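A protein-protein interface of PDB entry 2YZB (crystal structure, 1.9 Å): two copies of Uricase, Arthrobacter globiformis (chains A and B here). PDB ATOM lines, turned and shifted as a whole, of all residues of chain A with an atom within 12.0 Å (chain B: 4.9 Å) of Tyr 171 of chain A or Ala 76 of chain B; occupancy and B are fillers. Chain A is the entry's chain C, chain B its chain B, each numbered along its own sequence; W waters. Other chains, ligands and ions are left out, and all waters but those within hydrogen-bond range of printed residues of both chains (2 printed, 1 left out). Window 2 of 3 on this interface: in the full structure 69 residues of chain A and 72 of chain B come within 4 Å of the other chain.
The side-chain hydroxyl (OG1) of Thr 172 of chain A lies within hydrogen-bond range of the side-chain hydroxyl (OG1) of Thr 69 of chain B.
O of Tyr 171 of chain A lies within hydrogen-bond range of ND2 of Asn 72 of chain B.
The side-chain amide nitrogen (ND2) of Asn 72 of chain B is in hydrogen-bond range of the side-chain hydroxyl (OG1) of Thr 173 of chain A, at 3.2 Å.
The side-chain hydroxyl of Thr 73 of chain B is in hydrogen-bond range of the backbone carbonyl oxygen of Thr 69 of chain B, 2.8 Å away.
OD1 of Asp 169 of chain A sits close to N of Tyr 171 of chain A.
The side-chain carboxylate (OD1) of Asp 169 of chain A is in hydrogen-bond range of the side-chain hydroxyl (OG1) of Thr 172 of chain A.
The backbone carbonyl oxygen (O) of Thr 173 of chain A lies within hydrogen-bond range of the side-chain amide nitrogen (NE2) of Gln 175 of chain A (3.3 Å).
Among the printed residues, pairs that only touch across the chains: Asp 169 of chain A with Thr 69 of chain B, Tyr 171 of chain A with Ala 76 of chain B, Tyr 171 of chain A with Thr 73 of chain B, Tyr 171 of chain A with Phe 77 of chain B, Tyr 171 of chain A with Thr 69 of chain B and Tyr 171 of chain A with His 95 of chain B.
Tyr 171 of chain A touches just these residues of chain B: Thr 69, Asn 72, Thr 73, Ala 76, Phe 77 and His 95.
Ala 76 of chain B touches one residue of chain A.
Thr 69 of chain B touches just these residues of chain A: Asp 169, Tyr 171 and Thr 172.
Thr 73 of chain B touches one residue of chain A.
No residue of chain A comes within 4 Å of Val 74 of chain B.
Of chain A, only Tyr 171 (3.6 Å) comes within 4 Å of Phe 77 of chain B.
No residue of chain A comes within 4 Å of Ala 78 of chain B.
Of the printed residues of chain A, His 95 of chain B touches Tyr 171.
Of the printed residues of chain B, Thr 173 of chain A touches Asn 72.
Printed residues of chain B within 4 Å of Thr 172 of chain A: Thr 69.
Of the printed residues of chain B, Asp 169 of chain A touches Thr 69.
Phe 163 of chain A touches none of the printed residues of chain B.
Pro 167 of chain A touches none of the printed residues of chain B.
The nearest residue of chain A that does not touch Ala 76 of chain B is Lys 170 of chain A (7.3 Å).
Of the 12 printed residues of chain A, 4 touch a printed residue of chain B.
Hydrophobic or aromatic side chains of chain A that line the printed part of chain B: Tyr 171.
Printed residues of chain B that touch a printed residue of chain A: Thr 69, Asn 72, Thr 73, Ala 76, Phe 77 and His 95.
Among the printed residues, no Asp or Glu carboxylate lies within 4 Å of a Lys or Arg side-chain nitrogen of the other chain.
No position is printed for both chains.
Of the 9 pairs that touch across the chains among the printed residues, none has its exchanged pair printed and touching as well.
Water W2 bridges the backbone carbonyl oxygen of Pro 167 of chain A (2.6 Å) and the side-chain hydroxyl of Thr 69 of chain B (3.2 Å).
Water W1 lies within hydrogen-bond range of the side-chain hydroxyl of Thr 73 of chain B (2.8 Å), the side-chain carboxylate of Asp 169 of chain A (2.8 Å) and a ring nitrogen (NE2) of His 95 of chain B (3.0 Å).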
ATOM      1  N   PHE A 163      -9.063  33.786 -33.565  1.00  0.00           N
ATOM      2  CA  PHE A 163      -8.258  33.781 -32.356  1.00  0.00           C
ATOM      3  C   PHE A 163      -6.786  33.866 -32.724  1.00  0.00           C
ATOM      4  O   PHE A 163      -6.178  32.885 -33.153  1.00  0.00           O
ATOM      5  CB  PHE A 163      -8.495  32.536 -31.500  1.00  0.00           C
ATOM      6  CG  PHE A 163      -7.863  32.628 -30.143  1.00  0.00           C
ATOM      7  CD1 PHE A 163      -8.282  33.599 -29.237  1.00  0.00           C
ATOM      8  CD2 PHE A 163      -6.811  31.792 -29.786  1.00  0.00           C
ATOM      9  CE1 PHE A 163      -7.665  33.740 -27.998  1.00  0.00           C
ATOM     10  CE2 PHE A 163      -6.183  31.925 -28.544  1.00  0.00           C
ATOM     11  CZ  PHE A 163      -6.611  32.903 -27.651  1.00  0.00           C
ATOM     12  N   PHE A 166      -2.344  36.241 -29.526  1.00  0.00           N
ATOM     13  CA  PHE A 166      -2.061  35.833 -28.153  1.00  0.00           C
ATOM     14  C   PHE A 166      -0.566  35.589 -27.974  1.00  0.00           C
ATOM     15  O   PHE A 166       0.132  35.223 -28.920  1.00  0.00           O
ATOM     16  CB  PHE A 166      -2.840  34.563 -27.782  1.00  0.00           C
ATOM     17  CG  PHE A 166      -2.675  33.431 -28.759  1.00  0.00           C
ATOM     18  CD1 PHE A 166      -3.481  33.348 -29.889  1.00  0.00           C
ATOM     19  CD2 PHE A 166      -1.721  32.443 -28.543  1.00  0.00           C
ATOM     20  CE1 PHE A 166      -3.340  32.296 -30.787  1.00  0.00           C
ATOM     21  CE2 PHE A 166      -1.571  31.386 -29.437  1.00  0.00           C
ATOM     22  CZ  PHE A 166      -2.383  31.312 -30.561  1.00  0.00           C
ATOM     23  N   PRO A 167      -0.052  35.801 -26.753  1.00  0.00           N
ATOM     24  CA  PRO A 167       1.375  35.590 -26.492  1.00  0.00           C
ATOM     25  C   PRO A 167       1.806  34.147 -26.759  1.00  0.00           C
ATOM     26  O   PRO A 167       0.997  33.223 -26.681  1.00  0.00           O
ATOM     27  CB  PRO A 167       1.518  35.990 -25.024  1.00  0.00           C
ATOM     28  CG  PRO A 167       0.164  35.672 -24.448  1.00  0.00           C
ATOM     29  CD  PRO A 167      -0.763  36.185 -25.520  1.00  0.00           C
ATOM     30  N   ARG A 168       3.081  33.960 -27.085  1.00  0.00           N
ATOM     31  CA  ARG A 168       3.604  32.628 -27.359  1.00  0.00           C
ATOM     32  C   ARG A 168       4.809  32.334 -26.478  1.00  0.00           C
ATOM     33  O   ARG A 168       5.866  32.946 -26.635  1.00  0.00           O
ATOM     34  CB  ARG A 168       4.014  32.511 -28.829  1.00  0.00           C
ATOM     35  CG  ARG A 168       2.942  32.946 -29.813  1.00  0.00           C
ATOM     36  CD  ARG A 168       3.337  32.584 -31.236  1.00  0.00           C
ATOM     37  NE  ARG A 168       3.260  31.144 -31.469  1.00  0.00           N
ATOM     38  CZ  ARG A 168       2.124  30.472 -31.635  1.00  0.00           C
ATOM     39  NH1 ARG A 168       0.961  31.106 -31.600  1.00  0.00           N
ATOM     40  NH2 ARG A 168       2.151  29.164 -31.836  1.00  0.00           N
ATOM     41  N   ASP A 169       4.656  31.392 -25.554  1.00  0.00           N
ATOM     42  CA  ASP A 169       5.753  31.040 -24.667  1.00  0.00           C
ATOM     43  C   ASP A 169       6.247  29.628 -24.962  1.00  0.00           C
ATOM     44  O   ASP A 169       5.825  28.999 -25.929  1.00  0.00           O
ATOM     45  CB  ASP A 169       5.310  31.166 -23.201  1.00  0.00           C
ATOM     46  CG  ASP A 169       4.370  30.050 -22.765  1.00  0.00           C
ATOM     47  OD1 ASP A 169       3.694  29.457 -23.631  1.00  0.00           O
ATOM     48  OD2 ASP A 169       4.302  29.777 -21.547  1.00  0.00           O
ATOM     49  N   LYS A 170       7.152  29.143 -24.122  1.00  0.00           N
ATOM     50  CA  LYS A 170       7.728  27.812 -24.260  1.00  0.00           C
ATOM     51  C   LYS A 170       6.699  26.698 -24.464  1.00  0.00           C
ATOM     52  O   LYS A 170       6.978  25.705 -25.134  1.00  0.00           O
ATOM     53  CB  LYS A 170       8.559  27.498 -23.016  1.00  0.00           C
ATOM     54  CG  LYS A 170       9.252  26.149 -23.032  1.00  0.00           C
ATOM     55  CD  LYS A 170      10.097  25.985 -21.784  1.00  0.00           C
ATOM     56  CE  LYS A 170      10.964  24.740 -21.843  1.00  0.00           C
ATOM     57  NZ  LYS A 170      11.881  24.677 -20.665  1.00  0.00           N
ATOM     58  N   TYR A 171       5.509  26.873 -23.895  1.00  0.00           N
ATOM     59  CA  TYR A 171       4.468  25.857 -23.978  1.00  0.00           C
ATOM     60  C   TYR A 171       3.339  26.148 -24.951  1.00  0.00           C
ATOM     61  O   TYR A 171       2.288  25.513 -24.884  1.00  0.00           O
ATOM     62  CB  TYR A 171       3.883  25.628 -22.585  1.00  0.00           C
ATOM     63  CG  TYR A 171       4.938  25.370 -21.539  1.00  0.00           C
ATOM     64  CD1 TYR A 171       5.712  24.213 -21.574  1.00  0.00           C
ATOM     65  CD2 TYR A 171       5.197  26.309 -20.542  1.00  0.00           C
ATOM     66  CE1 TYR A 171       6.724  23.996 -20.638  1.00  0.00           C
ATOM     67  CE2 TYR A 171       6.201  26.104 -19.605  1.00  0.00           C
ATOM     68  CZ  TYR A 171       6.961  24.950 -19.657  1.00  0.00           C
ATOM     69  OH  TYR A 171       7.953  24.749 -18.729  1.00  0.00           O
ATOM     70  N   THR A 172       3.548  27.095 -25.855  1.00  0.00           N
ATOM     71  CA  THR A 172       2.517  27.442 -26.824  1.00  0.00           C
ATOM     72  C   THR A 172       2.737  26.741 -28.156  1.00  0.00           C
ATOM     73  O   THR A 172       3.799  26.867 -28.761  1.00  0.00           O
ATOM     74  CB  THR A 172       2.478  28.959 -27.075  1.00  0.00           C
ATOM     75  OG1 THR A 172       2.348  29.645 -25.825  1.00  0.00           O
ATOM     76  CG2 THR A 172       1.297  29.322 -27.958  1.00  0.00           C
ATOM     77  N   THR A 173       1.728  26.002 -28.610  1.00  0.00           N
ATOM     78  CA  THR A 173       1.804  25.292 -29.881  1.00  0.00           C
ATOM     79  C   THR A 173       0.577  25.606 -30.727  1.00  0.00           C
ATOM     80  O   THR A 173       0.522  25.264 -31.907  1.00  0.00           O
ATOM     81  CB  THR A 173       1.871  23.763 -29.678  1.00  0.00           C
ATOM     82  OG1 THR A 173       0.681  23.309 -29.017  1.00  0.00           O
ATOM     83  CG2 THR A 173       3.081  23.393 -28.843  1.00  0.00           C
ATOM     84  N   LEU A 174      -0.409  26.259 -30.121  1.00  0.00           N
ATOM     85  CA  LEU A 174      -1.640  26.599 -30.832  1.00  0.00           C
ATOM     86  C   LEU A 174      -1.367  27.544 -31.997  1.00  0.00           C
ATOM     87  O   LEU A 174      -0.672  28.551 -31.847  1.00  0.00           O
ATOM     88  CB  LEU A 174      -2.650  27.247 -29.878  1.00  0.00           C
ATOM     89  CG  LEU A 174      -3.962  27.734 -30.508  1.00  0.00           C
ATOM     90  CD1 LEU A 174      -4.764  26.544 -31.017  1.00  0.00           C
ATOM     91  CD2 LEU A 174      -4.773  28.514 -29.485  1.00  0.00           C
ATOM     92  N   GLN A 175      -1.911  27.210 -33.162  1.00  0.00           N
ATOM     93  CA  GLN A 175      -1.722  28.046 -34.335  1.00  0.00           C
ATOM     94  C   GLN A 175      -2.800  29.115 -34.409  1.00  0.00           C
ATOM     95  O   GLN A 175      -3.966  28.854 -34.115  1.00  0.00           O
ATOM     96  CB  GLN A 175      -1.737  27.192 -35.603  1.00  0.00           C
ATOM     97  CG  GLN A 175      -0.506  26.313 -35.741  1.00  0.00           C
ATOM     98  CD  GLN A 175       0.791  27.104 -35.598  1.00  0.00           C
ATOM     99  OE1 GLN A 175       1.052  28.039 -36.360  1.00  0.00           O
ATOM    100  NE2 GLN A 175       1.610  26.731 -34.615  1.00  0.00           N
ATOM    101  N   GLU A 176      -2.407  30.325 -34.782  1.00  0.00           N
ATOM    102  CA  GLU A 176      -3.369  31.413 -34.895  1.00  0.00           C
ATOM    103  C   GLU A 176      -4.331  31.073 -36.022  1.00  0.00           C
ATOM    104  O   GLU A 176      -3.973  30.350 -36.948  1.00  0.00           O
ATOM    105  CB  GLU A 176      -2.659  32.731 -35.212  1.00  0.00           C
ATOM    106  CG  GLU A 176      -1.590  33.134 -34.213  1.00  0.00           C
ATOM    107  CD  GLU A 176      -1.180  34.580 -34.377  1.00  0.00           C
ATOM    108  OE1 GLU A 176      -1.015  35.016 -35.539  1.00  0.00           O
ATOM    109  OE2 GLU A 176      -1.015  35.280 -33.354  1.00  0.00           O
ATOM    110  N   THR B  69      -2.476  26.631 -24.206  1.00  0.00           N
ATOM    111  CA  THR B  69      -1.142  26.746 -23.621  1.00  0.00           C
ATOM    112  C   THR B  69      -1.207  26.307 -22.160  1.00  0.00           C
ATOM    113  O   THR B  69      -0.302  25.631 -21.661  1.00  0.00           O
ATOM    114  CB  THR B  69      -0.617  28.200 -23.687  1.00  0.00           C
ATOM    115  OG1 THR B  69      -0.402  28.568 -25.056  1.00  0.00           O
ATOM    116  CG2 THR B  69       0.699  28.341 -22.902  1.00  0.00           C
ATOM    117  N   ASN B  72      -1.138  22.614 -22.122  1.00  0.00           N
ATOM    118  CA  ASN B  72       0.204  22.105 -22.399  1.00  0.00           C
ATOM    119  C   ASN B  72       1.090  22.174 -21.168  1.00  0.00           C
ATOM    120  O   ASN B  72       1.848  21.243 -20.884  1.00  0.00           O
ATOM    121  CB  ASN B  72       0.876  22.891 -23.529  1.00  0.00           C
ATOM    122  CG  ASN B  72       0.294  22.573 -24.884  1.00  0.00           C
ATOM    123  OD1 ASN B  72      -0.407  21.569 -25.053  1.00  0.00           O
ATOM    124  ND2 ASN B  72       0.581  23.423 -25.866  1.00  0.00           N
ATOM    125  N   THR B  73       0.995  23.287 -20.445  1.00  0.00           N
ATOM    126  CA  THR B  73       1.795  23.487 -19.248  1.00  0.00           C
ATOM    127  C   THR B  73       1.490  22.434 -18.181  1.00  0.00           C
ATOM    128  O   THR B  73       2.395  21.958 -17.496  1.00  0.00           O
ATOM    129  CB  THR B  73       1.554  24.892 -18.673  1.00  0.00           C
ATOM    130  OG1 THR B  73       1.738  25.866 -19.710  1.00  0.00           O
ATOM    131  CG2 THR B  73       2.528  25.180 -17.543  1.00  0.00           C
ATOM    132  N   VAL B  74       0.217  22.067 -18.034  1.00  0.00           N
ATOM    133  CA  VAL B  74      -0.153  21.049 -17.055  1.00  0.00           C
ATOM    134  C   VAL B  74       0.605  19.750 -17.360  1.00  0.00           C
ATOM    135  O   VAL B  74       1.233  19.156 -16.480  1.00  0.00           O
ATOM    136  CB  VAL B  74      -1.686  20.771 -17.074  1.00  0.00           C
ATOM    137  CG1 VAL B  74      -2.008  19.496 -16.290  1.00  0.00           C
ATOM    138  CG2 VAL B  74      -2.439  21.945 -16.465  1.00  0.00           C
ATOM    139  N   TYR B  75       0.561  19.317 -18.612  1.00  0.00           N
ATOM    140  CA  TYR B  75       1.250  18.089 -18.993  1.00  0.00           C
ATOM    141  C   TYR B  75       2.769  18.220 -18.903  1.00  0.00           C
ATOM    142  O   TYR B  75       3.454  17.281 -18.491  1.00  0.00           O
ATOM    143  CB  TYR B  75       0.828  17.672 -20.408  1.00  0.00           C
ATOM    144  CG  TYR B  75      -0.600  17.169 -20.467  1.00  0.00           C
ATOM    145  CD1 TYR B  75      -0.965  15.992 -19.811  1.00  0.00           C
ATOM    146  CD2 TYR B  75      -1.589  17.881 -21.147  1.00  0.00           C
ATOM    147  CE1 TYR B  75      -2.275  15.537 -19.821  1.00  0.00           C
ATOM    148  CE2 TYR B  75      -2.910  17.433 -21.169  1.00  0.00           C
ATOM    149  CZ  TYR B  75      -3.246  16.258 -20.499  1.00  0.00           C
ATOM    150  OH  TYR B  75      -4.544  15.805 -20.491  1.00  0.00           O
ATOM    151  N   ALA B  76       3.298  19.382 -19.271  1.00  0.00           N
ATOM    152  CA  ALA B  76       4.746  19.584 -19.223  1.00  0.00           C
ATOM    153  C   ALA B  76       5.246  19.513 -17.780  1.00  0.00           C
ATOM    154  O   ALA B  76       6.269  18.888 -17.505  1.00  0.00           O
ATOM    155  CB  ALA B  76       5.118  20.931 -19.850  1.00  0.00           C
ATOM    156  N   PHE B  77       4.521  20.147 -16.860  1.00  0.00           N
ATOM    157  CA  PHE B  77       4.908  20.121 -15.455  1.00  0.00           C
ATOM    158  C   PHE B  77       4.763  18.728 -14.845  1.00  0.00           C
ATOM    159  O   PHE B  77       5.519  18.364 -13.946  1.00  0.00           O
ATOM    160  CB  PHE B  77       4.074  21.115 -14.637  1.00  0.00           C
ATOM    161  CG  PHE B  77       4.546  22.542 -14.737  1.00  0.00           C
ATOM    162  CD1 PHE B  77       4.086  23.498 -13.834  1.00  0.00           C
ATOM    163  CD2 PHE B  77       5.448  22.932 -15.720  1.00  0.00           C
ATOM    164  CE1 PHE B  77       4.522  24.822 -13.908  1.00  0.00           C
ATOM    165  CE2 PHE B  77       5.893  24.255 -15.806  1.00  0.00           C
ATOM    166  CZ  PHE B  77       5.429  25.200 -14.896  1.00  0.00           C
ATOM    167  N   ALA B  78       3.800  17.950 -15.329  1.00  0.00           N
ATOM    168  CA  ALA B  78       3.579  16.604 -14.801  1.00  0.00           C
ATOM    169  C   ALA B  78       4.786  15.694 -15.012  1.00  0.00           C
ATOM    170  O   ALA B  78       5.016  14.768 -14.235  1.00  0.00           O
ATOM    171  CB  ALA B  78       2.322  15.977 -15.445  1.00  0.00           C
ATOM    172  N   ARG B  79       5.551  15.962 -16.067  1.00  0.00           N
ATOM    173  CA  ARG B  79       6.740  15.174 -16.395  1.00  0.00           C
ATOM    174  C   ARG B  79       7.738  15.098 -15.242  1.00  0.00           C
ATOM    175  O   ARG B  79       8.421  14.089 -15.069  1.00  0.00           O
ATOM    176  CB  ARG B  79       7.441  15.769 -17.621  1.00  0.00           C
ATOM    177  CG  ARG B  79       8.801  15.140 -17.945  1.00  0.00           C
ATOM    178  CD  ARG B  79       8.675  13.701 -18.441  1.00  0.00           C
ATOM    179  NE  ARG B  79       9.978  13.099 -18.733  1.00  0.00           N
ATOM    180  CZ  ARG B  79      10.781  12.556 -17.817  1.00  0.00           C
ATOM    181  NH1 ARG B  79      10.418  12.534 -16.540  1.00  0.00           N
ATOM    182  NH2 ARG B  79      11.948  12.034 -18.181  1.00  0.00           N
ATOM    183  N   ASP B  80       7.826  16.169 -14.461  1.00  0.00           N
ATOM    184  CA  ASP B  80       8.756  16.219 -13.337  1.00  0.00           C
ATOM    185  C   ASP B  80       8.238  15.482 -12.116  1.00  0.00           C
ATOM    186  O   ASP B  80       8.982  15.228 -11.168  1.00  0.00           O
ATOM    187  CB  ASP B  80       9.047  17.672 -12.972  1.00  0.00           C
ATOM    188  CG  ASP B  80       9.625  18.447 -14.133  1.00  0.00           C
ATOM    189  OD1 ASP B  80      10.693  18.035 -14.638  1.00  0.00           O
ATOM    190  OD2 ASP B  80       9.012  19.458 -14.543  1.00  0.00           O
ATOM    191  N   HIS B  95       3.809  29.399 -11.375  1.00  0.00           N
ATOM    192  CA  HIS B  95       4.249  29.586 -12.747  1.00  0.00           C
ATOM    193  C   HIS B  95       3.498  30.686 -13.494  1.00  0.00           C
ATOM    194  O   HIS B  95       4.113  31.545 -14.119  1.00  0.00           O
ATOM    195  CB  HIS B  95       4.108  28.281 -13.531  1.00  0.00           C
ATOM    196  CG  HIS B  95       4.294  28.451 -15.006  1.00  0.00           C
ATOM    197  ND1 HIS B  95       5.518  28.728 -15.575  1.00  0.00           N
ATOM    198  CD2 HIS B  95       3.401  28.436 -16.023  1.00  0.00           C
ATOM    199  CE1 HIS B  95       5.371  28.879 -16.879  1.00  0.00           C
ATOM    200  NE2 HIS B  95       4.095  28.707 -17.177  1.00  0.00           N
HETATM  201  O   HOH W   1       2.555  28.520 -19.688  1.00  0.00           O
HETATM  202  O   HOH W   2      -0.650  31.711 -25.277  1.00  0.00           O
